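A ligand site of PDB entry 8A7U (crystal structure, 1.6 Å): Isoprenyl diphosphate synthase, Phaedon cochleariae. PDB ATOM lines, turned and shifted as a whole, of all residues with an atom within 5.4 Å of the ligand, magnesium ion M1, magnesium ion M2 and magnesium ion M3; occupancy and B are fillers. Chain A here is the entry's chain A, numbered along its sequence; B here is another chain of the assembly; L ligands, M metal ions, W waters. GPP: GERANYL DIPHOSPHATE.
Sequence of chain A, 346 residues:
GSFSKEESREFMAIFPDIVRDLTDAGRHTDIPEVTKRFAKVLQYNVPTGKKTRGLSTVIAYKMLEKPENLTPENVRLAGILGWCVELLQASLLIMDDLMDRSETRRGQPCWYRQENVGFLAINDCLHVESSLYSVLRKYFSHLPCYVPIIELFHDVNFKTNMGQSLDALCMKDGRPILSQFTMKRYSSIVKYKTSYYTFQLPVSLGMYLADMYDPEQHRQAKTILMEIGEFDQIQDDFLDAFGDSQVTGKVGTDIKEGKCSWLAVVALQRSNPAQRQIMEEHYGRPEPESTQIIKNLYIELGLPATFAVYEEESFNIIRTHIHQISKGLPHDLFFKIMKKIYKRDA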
ATOM      1  N   LEU A  92      23.764 -20.104 -13.585  1.00  0.00           N
ATOM      2  CA  LEU A  92      24.426 -21.380 -13.297  1.00  0.00           C
ATOM      3  C   LEU A  92      23.788 -22.448 -14.193  1.00  0.00           C
ATOM      4  O   LEU A  92      24.529 -23.306 -14.713  1.00  0.00           O
ATOM      5  CB  LEU A  92      24.245 -21.749 -11.841  1.00  0.00           C
ATOM      6  CG  LEU A  92      24.923 -20.798 -10.843  1.00  0.00           C
ATOM      7  CD1 LEU A  92      24.435 -21.163  -9.455  1.00  0.00           C
ATOM      8  CD2 LEU A  92      26.438 -20.837 -10.965  1.00  0.00           C
ATOM      9  N   LEU A  93      22.474 -22.410 -14.339  1.00  0.00           N
ATOM     10  CA  LEU A  93      21.829 -23.511 -15.081  1.00  0.00           C
ATOM     11  C   LEU A  93      22.038 -23.338 -16.570  1.00  0.00           C
ATOM     12  O   LEU A  93      22.186 -24.391 -17.231  1.00  0.00           O
ATOM     13  CB  LEU A  93      20.363 -23.543 -14.699  1.00  0.00           C
ATOM     14  CG  LEU A  93      20.120 -23.773 -13.184  1.00  0.00           C
ATOM     15  CD1 LEU A  93      18.636 -23.889 -12.907  1.00  0.00           C
ATOM     16  CD2 LEU A  93      20.862 -25.013 -12.649  1.00  0.00           C
ATOM     17  N   MET A  95      24.737 -22.369 -17.934  1.00  0.00           N
ATOM     18  CA  MET A  95      26.080 -22.942 -18.135  1.00  0.00           C
ATOM     19  C   MET A  95      26.060 -24.457 -17.909  1.00  0.00           C
ATOM     20  O   MET A  95      26.707 -25.172 -18.717  1.00  0.00           O
ATOM     21  CB  MET A  95      27.101 -22.297 -17.196  1.00  0.00           C
ATOM     22  CG  MET A  95      28.521 -22.849 -17.371  1.00  0.00           C
ATOM     23  SD  MET A  95      29.758 -21.828 -16.554  1.00  0.00           S
ATOM     24  CE  MET A  95      30.048 -20.606 -17.836  1.00  0.00           C
ATOM     25  N   ASP A  96      25.425 -24.916 -16.841  1.00  0.00           N
ATOM     26  CA  ASP A  96      25.419 -26.370 -16.582  1.00  0.00           C
ATOM     27  C   ASP A  96      24.782 -27.097 -17.761  1.00  0.00           C
ATOM     28  O   ASP A  96      25.265 -28.154 -18.113  1.00  0.00           O
ATOM     29  CB  ASP A  96      24.694 -26.687 -15.283  1.00  0.00           C
ATOM     30  CG  ASP A  96      24.622 -28.167 -15.045  1.00  0.00           C
ATOM     31  OD1 ASP A  96      25.610 -28.717 -14.577  1.00  0.00           O
ATOM     32  OD2 ASP A  96      23.553 -28.738 -15.405  1.00  0.00           O
ATOM     33  N   ASP A  97      23.722 -26.559 -18.326  1.00  0.00           N
ATOM     34  CA  ASP A  97      23.061 -27.268 -19.459  1.00  0.00           C
ATOM     35  C   ASP A  97      23.999 -27.397 -20.630  1.00  0.00           C
ATOM     36  O   ASP A  97      23.924 -28.444 -21.356  1.00  0.00           O
ATOM     37  CB  ASP A  97      21.724 -26.625 -19.779  1.00  0.00           C
ATOM     38  CG  ASP A  97      20.660 -26.916 -18.730  1.00  0.00           C
ATOM     39  OD1 ASP A  97      20.739 -27.999 -18.074  1.00  0.00           O
ATOM     40  OD2 ASP A  97      19.719 -26.089 -18.579  1.00  0.00           O
ATOM     41  N   MET A  99      27.297 -27.484 -20.419  1.00  0.00           N
ATOM     42  CA  MET A  99      28.323 -28.465 -19.977  1.00  0.00           C
ATOM     43  C   MET A  99      27.802 -29.916 -20.116  1.00  0.00           C
ATOM     44  O   MET A  99      28.635 -30.785 -20.464  1.00  0.00           O
ATOM     45  CB  MET A  99      28.712 -28.169 -18.522  1.00  0.00           C
ATOM     46  CG  MET A  99      29.532 -26.884 -18.471  1.00  0.00           C
ATOM     47  SD  MET A  99      30.057 -26.397 -16.815  1.00  0.00           S
ATOM     48  CE  MET A  99      31.131 -27.738 -16.335  1.00  0.00           C
ATOM     49  N   ASP A 100      26.535 -30.154 -19.748  1.00  0.00           N
ATOM     50  CA  ASP A 100      25.907 -31.510 -19.689  1.00  0.00           C
ATOM     51  C   ASP A 100      25.308 -31.864 -21.051  1.00  0.00           C
ATOM     52  O   ASP A 100      24.830 -33.012 -21.202  1.00  0.00           O
ATOM     53  CB  ASP A 100      24.950 -31.590 -18.499  1.00  0.00           C
ATOM     54  CG  ASP A 100      25.725 -31.406 -17.196  1.00  0.00           C
ATOM     55  OD1 ASP A 100      26.970 -31.646 -17.242  1.00  0.00           O
ATOM     56  OD2 ASP A 100      25.066 -31.075 -16.151  1.00  0.00           O
ATOM     57  N   SER A 102      22.453 -31.044 -22.098  1.00  0.00           N
ATOM     58  CA  SER A 102      21.046 -31.413 -21.811  1.00  0.00           C
ATOM     59  C   SER A 102      20.087 -30.910 -22.896  1.00  0.00           C
ATOM     60  O   SER A 102      20.349 -29.920 -23.585  1.00  0.00           O
ATOM     61  CB  SER A 102      20.667 -30.941 -20.442  1.00  0.00           C
ATOM     62  OG  SER A 102      21.379 -31.672 -19.463  1.00  0.00           O
ATOM     63  N   ARG A 105      15.269 -28.145 -19.566  1.00  0.00           N
ATOM     64  CA  ARG A 105      15.443 -27.633 -18.174  1.00  0.00           C
ATOM     65  C   ARG A 105      14.060 -27.114 -17.784  1.00  0.00           C
ATOM     66  O   ARG A 105      13.511 -26.285 -18.585  1.00  0.00           O
ATOM     67  CB  ARG A 105      16.565 -26.585 -18.180  1.00  0.00           C
ATOM     68  CG  ARG A 105      16.628 -25.627 -16.985  1.00  0.00           C
ATOM     69  CD  ARG A 105      17.222 -26.220 -15.739  1.00  0.00           C
ATOM     70  NE  ARG A 105      18.576 -26.657 -15.929  1.00  0.00           N
ATOM     71  CZ  ARG A 105      19.209 -27.481 -15.075  1.00  0.00           C
ATOM     72  NH1 ARG A 105      18.576 -27.911 -13.990  1.00  0.00           N
ATOM     73  NH2 ARG A 105      20.446 -27.851 -15.316  1.00  0.00           N
ATOM     74  N   THR A 160      30.300 -22.213  -5.493  1.00  0.00           N
ATOM     75  CA  THR A 160      29.473 -23.046  -6.423  1.00  0.00           C
ATOM     76  C   THR A 160      30.351 -23.553  -7.552  1.00  0.00           C
ATOM     77  O   THR A 160      30.165 -24.724  -7.984  1.00  0.00           O
ATOM     78  CB  THR A 160      28.262 -22.253  -6.950  1.00  0.00           C
ATOM     79  OG1 THR A 160      27.492 -21.760  -5.863  1.00  0.00           O
ATOM     80  CG2 THR A 160      27.360 -23.139  -7.801  1.00  0.00           C
ATOM     81  N   ASN A 161      31.239 -22.746  -8.078  1.00  0.00           N
ATOM     82  CA  ASN A 161      32.236 -23.185  -9.094  1.00  0.00           C
ATOM     83  C   ASN A 161      33.093 -24.328  -8.585  1.00  0.00           C
ATOM     84  O   ASN A 161      33.393 -25.272  -9.351  1.00  0.00           O
ATOM     85  CB  ASN A 161      33.033 -22.017  -9.641  1.00  0.00           C
ATOM     86  CG  ASN A 161      32.268 -21.292 -10.717  1.00  0.00           C
ATOM     87  OD1 ASN A 161      32.296 -21.760 -11.867  1.00  0.00           O
ATOM     88  ND2 ASN A 161      31.591 -20.217 -10.395  1.00  0.00           N
ATOM     89  N   GLN A 164      30.923 -27.369  -8.843  1.00  0.00           N
ATOM     90  CA  GLN A 164      30.726 -27.842 -10.245  1.00  0.00           C
ATOM     91  C   GLN A 164      31.992 -28.534 -10.743  1.00  0.00           C
ATOM     92  O   GLN A 164      31.908 -29.582 -11.419  1.00  0.00           O
ATOM     93  CB  GLN A 164      30.385 -26.644 -11.126  1.00  0.00           C
ATOM     94  CG  GLN A 164      30.160 -26.999 -12.601  1.00  0.00           C
ATOM     95  CD  GLN A 164      28.810 -27.636 -12.867  1.00  0.00           C
ATOM     96  OE1 GLN A 164      28.244 -28.229 -11.949  1.00  0.00           O
ATOM     97  NE2 GLN A 164      28.258 -27.484 -14.103  1.00  0.00           N
ATOM     98  N   ASP A 167      32.350 -31.934  -9.123  1.00  0.00           N
ATOM     99  CA  ASP A 167      31.421 -32.858  -9.820  1.00  0.00           C
ATOM    100  C   ASP A 167      32.105 -33.326 -11.113  1.00  0.00           C
ATOM    101  O   ASP A 167      32.042 -34.546 -11.428  1.00  0.00           O
ATOM    102  CB  ASP A 167      30.088 -32.149 -10.049  1.00  0.00           C
ATOM    103  CG  ASP A 167      28.900 -33.012 -10.371  1.00  0.00           C
ATOM    104  OD1 ASP A 167      28.923 -34.178 -10.011  1.00  0.00           O
ATOM    105  OD2 ASP A 167      27.930 -32.456 -10.853  1.00  0.00           O
ATOM    106  N   LYS A 193      28.247 -27.271  -4.645  1.00  0.00           N
ATOM    107  CA  LYS A 193      27.523 -27.041  -5.915  1.00  0.00           C
ATOM    108  C   LYS A 193      26.087 -26.572  -5.704  1.00  0.00           C
ATOM    109  O   LYS A 193      25.579 -25.813  -6.570  1.00  0.00           O
ATOM    110  CB  LYS A 193      27.509 -28.328  -6.736  1.00  0.00           C
ATOM    111  CG  LYS A 193      27.088 -28.145  -8.176  1.00  0.00           C
ATOM    112  CD  LYS A 193      26.929 -29.435  -8.961  1.00  0.00           C
ATOM    113  CE  LYS A 193      25.700 -30.197  -8.505  1.00  0.00           C
ATOM    114  NZ  LYS A 193      25.548 -31.469  -9.224  1.00  0.00           N
ATOM    115  N   THR A 194      25.404 -27.008  -4.638  1.00  0.00           N
ATOM    116  CA  THR A 194      23.959 -26.722  -4.478  1.00  0.00           C
ATOM    117  C   THR A 194      23.621 -26.047  -3.158  1.00  0.00           C
ATOM    118  O   THR A 194      22.798 -25.106  -3.188  1.00  0.00           O
ATOM    119  CB  THR A 194      23.065 -27.924  -4.754  1.00  0.00           C
ATOM    120  OG1 THR A 194      23.348 -28.964  -3.842  1.00  0.00           O
ATOM    121  CG2 THR A 194      23.396 -28.409  -6.135  1.00  0.00           C
ATOM    122  N   TYR A 197      24.179 -22.054  -2.567  1.00  0.00           N
ATOM    123  CA  TYR A 197      23.321 -21.062  -3.266  1.00  0.00           C
ATOM    124  C   TYR A 197      21.849 -21.323  -2.988  1.00  0.00           C
ATOM    125  O   TYR A 197      21.039 -20.396  -3.070  1.00  0.00           O
ATOM    126  CB  TYR A 197      23.644 -20.953  -4.745  1.00  0.00           C
ATOM    127  CG  TYR A 197      22.853 -21.834  -5.667  1.00  0.00           C
ATOM    128  CD1 TYR A 197      21.646 -21.393  -6.160  1.00  0.00           C
ATOM    129  CD2 TYR A 197      23.270 -23.121  -6.007  1.00  0.00           C
ATOM    130  CE1 TYR A 197      20.855 -22.164  -7.001  1.00  0.00           C
ATOM    131  CE2 TYR A 197      22.524 -23.872  -6.905  1.00  0.00           C
ATOM    132  CZ  TYR A 197      21.304 -23.417  -7.361  1.00  0.00           C
ATOM    133  OH  TYR A 197      20.514 -24.154  -8.163  1.00  0.00           O
ATOM    134  N   THR A 253      17.029 -39.075 -15.750  1.00  0.00           N
ATOM    135  CA  THR A 253      18.139 -39.430 -16.665  1.00  0.00           C
ATOM    136  C   THR A 253      19.478 -39.463 -15.923  1.00  0.00           C
ATOM    137  O   THR A 253      20.519 -39.507 -16.595  1.00  0.00           O
ATOM    138  CB  THR A 253      18.187 -38.469 -17.857  1.00  0.00           C
ATOM    139  OG1 THR A 253      18.235 -37.148 -17.341  1.00  0.00           O
ATOM    140  CG2 THR A 253      16.976 -38.664 -18.754  1.00  0.00           C
ATOM    141  N   ASP A 254      19.474 -39.467 -14.587  1.00  0.00           N
ATOM    142  CA  ASP A 254      20.769 -39.393 -13.862  1.00  0.00           C
ATOM    143  C   ASP A 254      21.659 -40.581 -14.191  1.00  0.00           C
ATOM    144  O   ASP A 254      22.877 -40.399 -14.306  1.00  0.00           O
ATOM    145  CB  ASP A 254      20.579 -39.384 -12.345  1.00  0.00           C
ATOM    146  CG  ASP A 254      19.993 -38.107 -11.762  1.00  0.00           C
ATOM    147  OD1 ASP A 254      19.806 -37.126 -12.541  1.00  0.00           O
ATOM    148  OD2 ASP A 254      19.705 -38.116 -10.574  1.00  0.00           O
ATOM    149  N   GLU A 257      23.291 -40.171 -17.606  1.00  0.00           N
ATOM    150  CA  GLU A 257      24.187 -38.994 -17.518  1.00  0.00           C
ATOM    151  C   GLU A 257      25.455 -39.371 -16.738  1.00  0.00           C
ATOM    152  O   GLU A 257      26.404 -38.577 -16.736  1.00  0.00           O
ATOM    153  CB  GLU A 257      23.387 -37.836 -16.913  1.00  0.00           C
ATOM    154  CG  GLU A 257      22.350 -37.233 -17.835  1.00  0.00           C
ATOM    155  CD  GLU A 257      21.419 -36.160 -17.230  1.00  0.00           C
ATOM    156  OE1 GLU A 257      21.063 -35.233 -17.912  1.00  0.00           O
ATOM    157  OE2 GLU A 257      21.023 -36.265 -16.080  1.00  0.00           O
ATOM    158  N   LYS A 259      25.785 -39.499 -13.434  1.00  0.00           N
ATOM    159  CA  LYS A 259      25.932 -38.609 -12.256  1.00  0.00           C
ATOM    160  C   LYS A 259      26.479 -39.325 -11.040  1.00  0.00           C
ATOM    161  O   LYS A 259      26.188 -40.505 -10.827  1.00  0.00           O
ATOM    162  CB  LYS A 259      24.592 -37.995 -11.867  1.00  0.00           C
ATOM    163  CG  LYS A 259      24.202 -36.954 -12.894  1.00  0.00           C
ATOM    164  CD  LYS A 259      23.070 -36.262 -12.431  1.00  0.00           C
ATOM    165  CE  LYS A 259      22.582 -35.240 -13.411  1.00  0.00           C
ATOM    166  NZ  LYS A 259      21.326 -34.709 -12.835  1.00  0.00           N
ATOM    167  N   ASN B 123      33.235 -23.950 -16.969  1.00  0.00           N
ATOM    168  CA  ASN B 123      32.972 -23.026 -15.830  1.00  0.00           C
ATOM    169  C   ASN B 123      34.262 -22.377 -15.354  1.00  0.00           C
ATOM    170  O   ASN B 123      34.176 -21.474 -14.497  1.00  0.00           O
ATOM    171  CB  ASN B 123      32.239 -23.737 -14.700  1.00  0.00           C
ATOM    172  CG  ASN B 123      33.058 -24.811 -14.034  1.00  0.00           C
ATOM    173  OD1 ASN B 123      33.418 -25.802 -14.672  1.00  0.00           O
ATOM    174  ND2 ASN B 123      33.270 -24.666 -12.718  1.00  0.00           N
ATOM    175  N   LEU B 126      34.020 -18.553 -15.629  1.00  0.00           N
ATOM    176  CA  LEU B 126      33.182 -17.943 -14.586  1.00  0.00           C
ATOM    177  C   LEU B 126      33.954 -17.954 -13.271  1.00  0.00           C
ATOM    178  O   LEU B 126      33.944 -16.938 -12.565  1.00  0.00           O
ATOM    179  CB  LEU B 126      31.901 -18.734 -14.442  1.00  0.00           C
ATOM    180  CG  LEU B 126      30.948 -18.259 -13.354  1.00  0.00           C
ATOM    181  CD1 LEU B 126      30.434 -16.893 -13.720  1.00  0.00           C
ATOM    182  CD2 LEU B 126      29.796 -19.233 -13.219  1.00  0.00           C
HETATM  183  C1  GPP L   1      22.963 -28.690 -11.986  1.00  0.00           C
HETATM  184  O1  GPP L   1      23.420 -29.957 -11.452  1.00  0.00           O
HETATM  185  C2  GPP L   1      24.020 -27.638 -11.647  1.00  0.00           C
HETATM  186  C3  GPP L   1      24.011 -26.674 -10.717  1.00  0.00           C
HETATM  187  C4  GPP L   1      22.946 -26.519  -9.672  1.00  0.00           C
HETATM  188  C5  GPP L   1      25.130 -25.671 -10.585  1.00  0.00           C
HETATM  189  C6  GPP L   1      26.062 -25.506 -11.745  1.00  0.00           C
HETATM  190  C7  GPP L   1      27.257 -24.695 -11.391  1.00  0.00           C
HETATM  191  C8  GPP L   1      28.055 -23.993 -12.177  1.00  0.00           C
HETATM  192  C9  GPP L   1      27.846 -23.787 -13.641  1.00  0.00           C
HETATM  193  C10 GPP L   1      29.231 -23.243 -11.651  1.00  0.00           C
HETATM  194  PA  GPP L   1      23.391 -31.303 -12.320  1.00  0.00           P
HETATM  195  O1A GPP L   1      24.031 -31.053 -13.648  1.00  0.00           O
HETATM  196  O2A GPP L   1      23.995 -32.378 -11.493  1.00  0.00           O
HETATM  197  O3A GPP L   1      21.831 -31.653 -12.457  1.00  0.00           O
HETATM  198  PB  GPP L   1      20.681 -31.136 -13.451  1.00  0.00           P
HETATM  199  O1B GPP L   1      21.378 -30.443 -14.588  1.00  0.00           O
HETATM  200  O2B GPP L   1      19.812 -30.240 -12.602  1.00  0.00           O
HETATM  201  O3B GPP L   1      20.011 -32.433 -13.875  1.00  0.00           O
HETATM  202 MG    MG M   1      25.984 -30.758 -14.276  1.00  0.00          MG
HETATM  203 MG    MG M   2      23.092 -30.734 -15.630  1.00  0.00          MG
HETATM  204 MG    MG M   3      18.586 -33.026 -15.213  1.00  0.00          MG
HETATM  205 MG    MG M   4      18.053 -34.429  -9.648  1.00  0.00          MG
HETATM  206  O   HOH W   1      22.631 -32.668 -15.957  1.00  0.00           O
HETATM  207  O   HOH W   2      22.083 -33.931 -10.144  1.00  0.00           O
HETATM  208  O   HOH W   3      17.189 -33.199 -13.553  1.00  0.00           O
HETATM  209  O   HOH W   4      26.700 -30.426 -12.353  1.00  0.00           O
HETATM  210  O   HOH W   5      17.033 -33.673 -16.485  1.00  0.00           O
HETATM  211  O   HOH W   6      27.881 -30.396 -15.073  1.00  0.00           O
HETATM  212  O   HOH W   7      25.954 -34.045 -11.793  1.00  0.00           O
HETATM  213  O   HOH W   8      22.355 -31.049  -8.396  1.00  0.00           O
HETATM  214  O   HOH W   9      22.258 -30.158 -17.419  1.00  0.00           O
HETATM  215  O   HOH W  10      20.046 -30.289  -9.989  1.00  0.00           O
HETATM  216  O   HOH W  11      17.949 -31.057 -15.592  1.00  0.00           O
HETATM  217  O   HOH W  12      26.433 -32.783 -14.127  1.00  0.00           O
HETATM  218  O   HOH W  13      19.858 -32.918 -16.837  1.00  0.00           O
HETATM  219  O   HOH W  14      17.325 -30.994 -12.127  1.00  0.00           O
HETATM  220  O   HOH W  15      19.094 -35.030 -14.952  1.00  0.00           O
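Gln 164 touches magnesium ion M1.
Within 4 Å of magnesium ion M1: Asp 96, Asp 100 and Gln 164.
The nearest printed residue that does not touch magnesium ion M1 is Asp 167 (4.3 Å).
An oxygen (O3B) of the ligand binds magnesium ion M3 (2.0 Å).
Water W13 is bound to magnesium ion M3 (2.1 Å).
Magnesium ion M3 is bound by water W15 (2.1 Å).
Magnesium ion M3 is bound by water W11.
Water W5 is bound to magnesium ion M3 (2.1 Å).
Water W3 binds magnesium ion M3, at 2.2 Å.
Lys 259 touches magnesium ion M3.
Of the 22 residues printed, 1 comes within 4 Å of magnesium ion M3.
Arg 105 touches magnesium ion M2 (NH2 to MG, 3.9 Å).
The side-chain carboxylate (OD2) of Asp 96 sits close to the guanidinium group (NH2) of Arg 105 (3.2 Å).
The side-chain amide nitrogen of Gln 164 lies close to the side-chain carboxylate of Asp 96.
OE2 of Glu 257 lies within salt-bridge range of NZ of Lys 259, at 3.6 Å.
The side-chain amino group of Lys 259 is in salt-bridge range of the side-chain carboxylate of Asp 254, 2.9 Å away.
OD1 of Asp 97 is in salt-bridge range of NH2 of Arg 105.
The side-chain amino group of Lys 193 lies within salt-bridge range of the side-chain carboxylate of Asp 167.
The side-chain amide oxygen (OD1) of Asn 161 is in hydrogen-bond range of the side-chain amide nitrogen (ND2) of Asn 123 of chain B, 3.2 Å away.
The side-chain sulfur (SD) of Met 99 lies within hydrogen-bond range of the side-chain amide nitrogen (NE2) of Gln 164, 3.4 Å away.
NZ of Lys 259 is in salt-bridge range of O2A of the ligand (3.8 Å).
The guanidinium group of Arg 105 lies within salt-bridge range of an oxygen (O2B) of the ligand.
NZ of Lys 193 is in salt-bridge range of O2A of the ligand, 2.9 Å away.
Water W6 bridges the side-chain carboxylate (OD1) of Asp 100 (2.7 Å) and the side-chain amide nitrogen (NE2) of Gln 164 (3.1 Å).
Water W9 bridges OG of Ser 102 (2.7 Å) and OD1 of Asp 97 (2.7 Å).
Water W13 lies within hydrogen-bond range of OE1 of Glu 257 and OG of Ser 102.
Water W7 bridges O2A of the ligand (2.6 Å) and OD2 of Asp 167 (2.7 Å).
Water W2 lies within hydrogen-bond range of an oxygen (O2A) of the ligand (2.8 Å) and the side-chain amino group (NZ) of Lys 259 (2.9 Å).
Water W8 lies within hydrogen-bond range of NZ of Lys 193 (3.3 Å) and O1 of the ligand (3.4 Å).
Merely in contact with the ligand: Asn 161, Gln 164, Leu 92, Tyr 197, Met 95, Thr 160, Leu 93 and Asp 167.
Hydrophobic or aromatic side chains that line the ligand: Leu 92, Leu 93, Met 95 and Tyr 197.
Within 4 Å of the ligand: Leu 92, Leu 93, Met 95, Asp 96, Asp 100, Arg 105, Thr 160, Asn 161, Gln 164, Asp 167, Lys 193, Tyr 197 and Lys 259.
Magnesium ion M1 is bound by O1A of the ligand (2.1 Å), water W4 (2.1 Å), water W12 (2.1 Å), water W6 (2.1 Å), OD1 of Asp 96 (2.1 Å) and OD2 of Asp 100 (2.1 Å).
Magnesium ion M1 has six donor atoms within binding distance.
Magnesium ion M2 is bound by water W1, 2.0 Å away.
Magnesium ion M2 is bound by an oxygen (O1B) of the ligand (2.0 Å).
Water W9 binds magnesium ion M2.
Magnesium ion M2 is bound by OD2 of Asp 96 (2.1 Å).
Magnesium ion M2 is bound by the side-chain carboxylate (OD2) of Asp 100.
Magnesium ion M2 is bound by an oxygen (O1A) of the ligand, at 2.2 Å.
Magnesium ion M2 has six donor atoms within binding distance.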
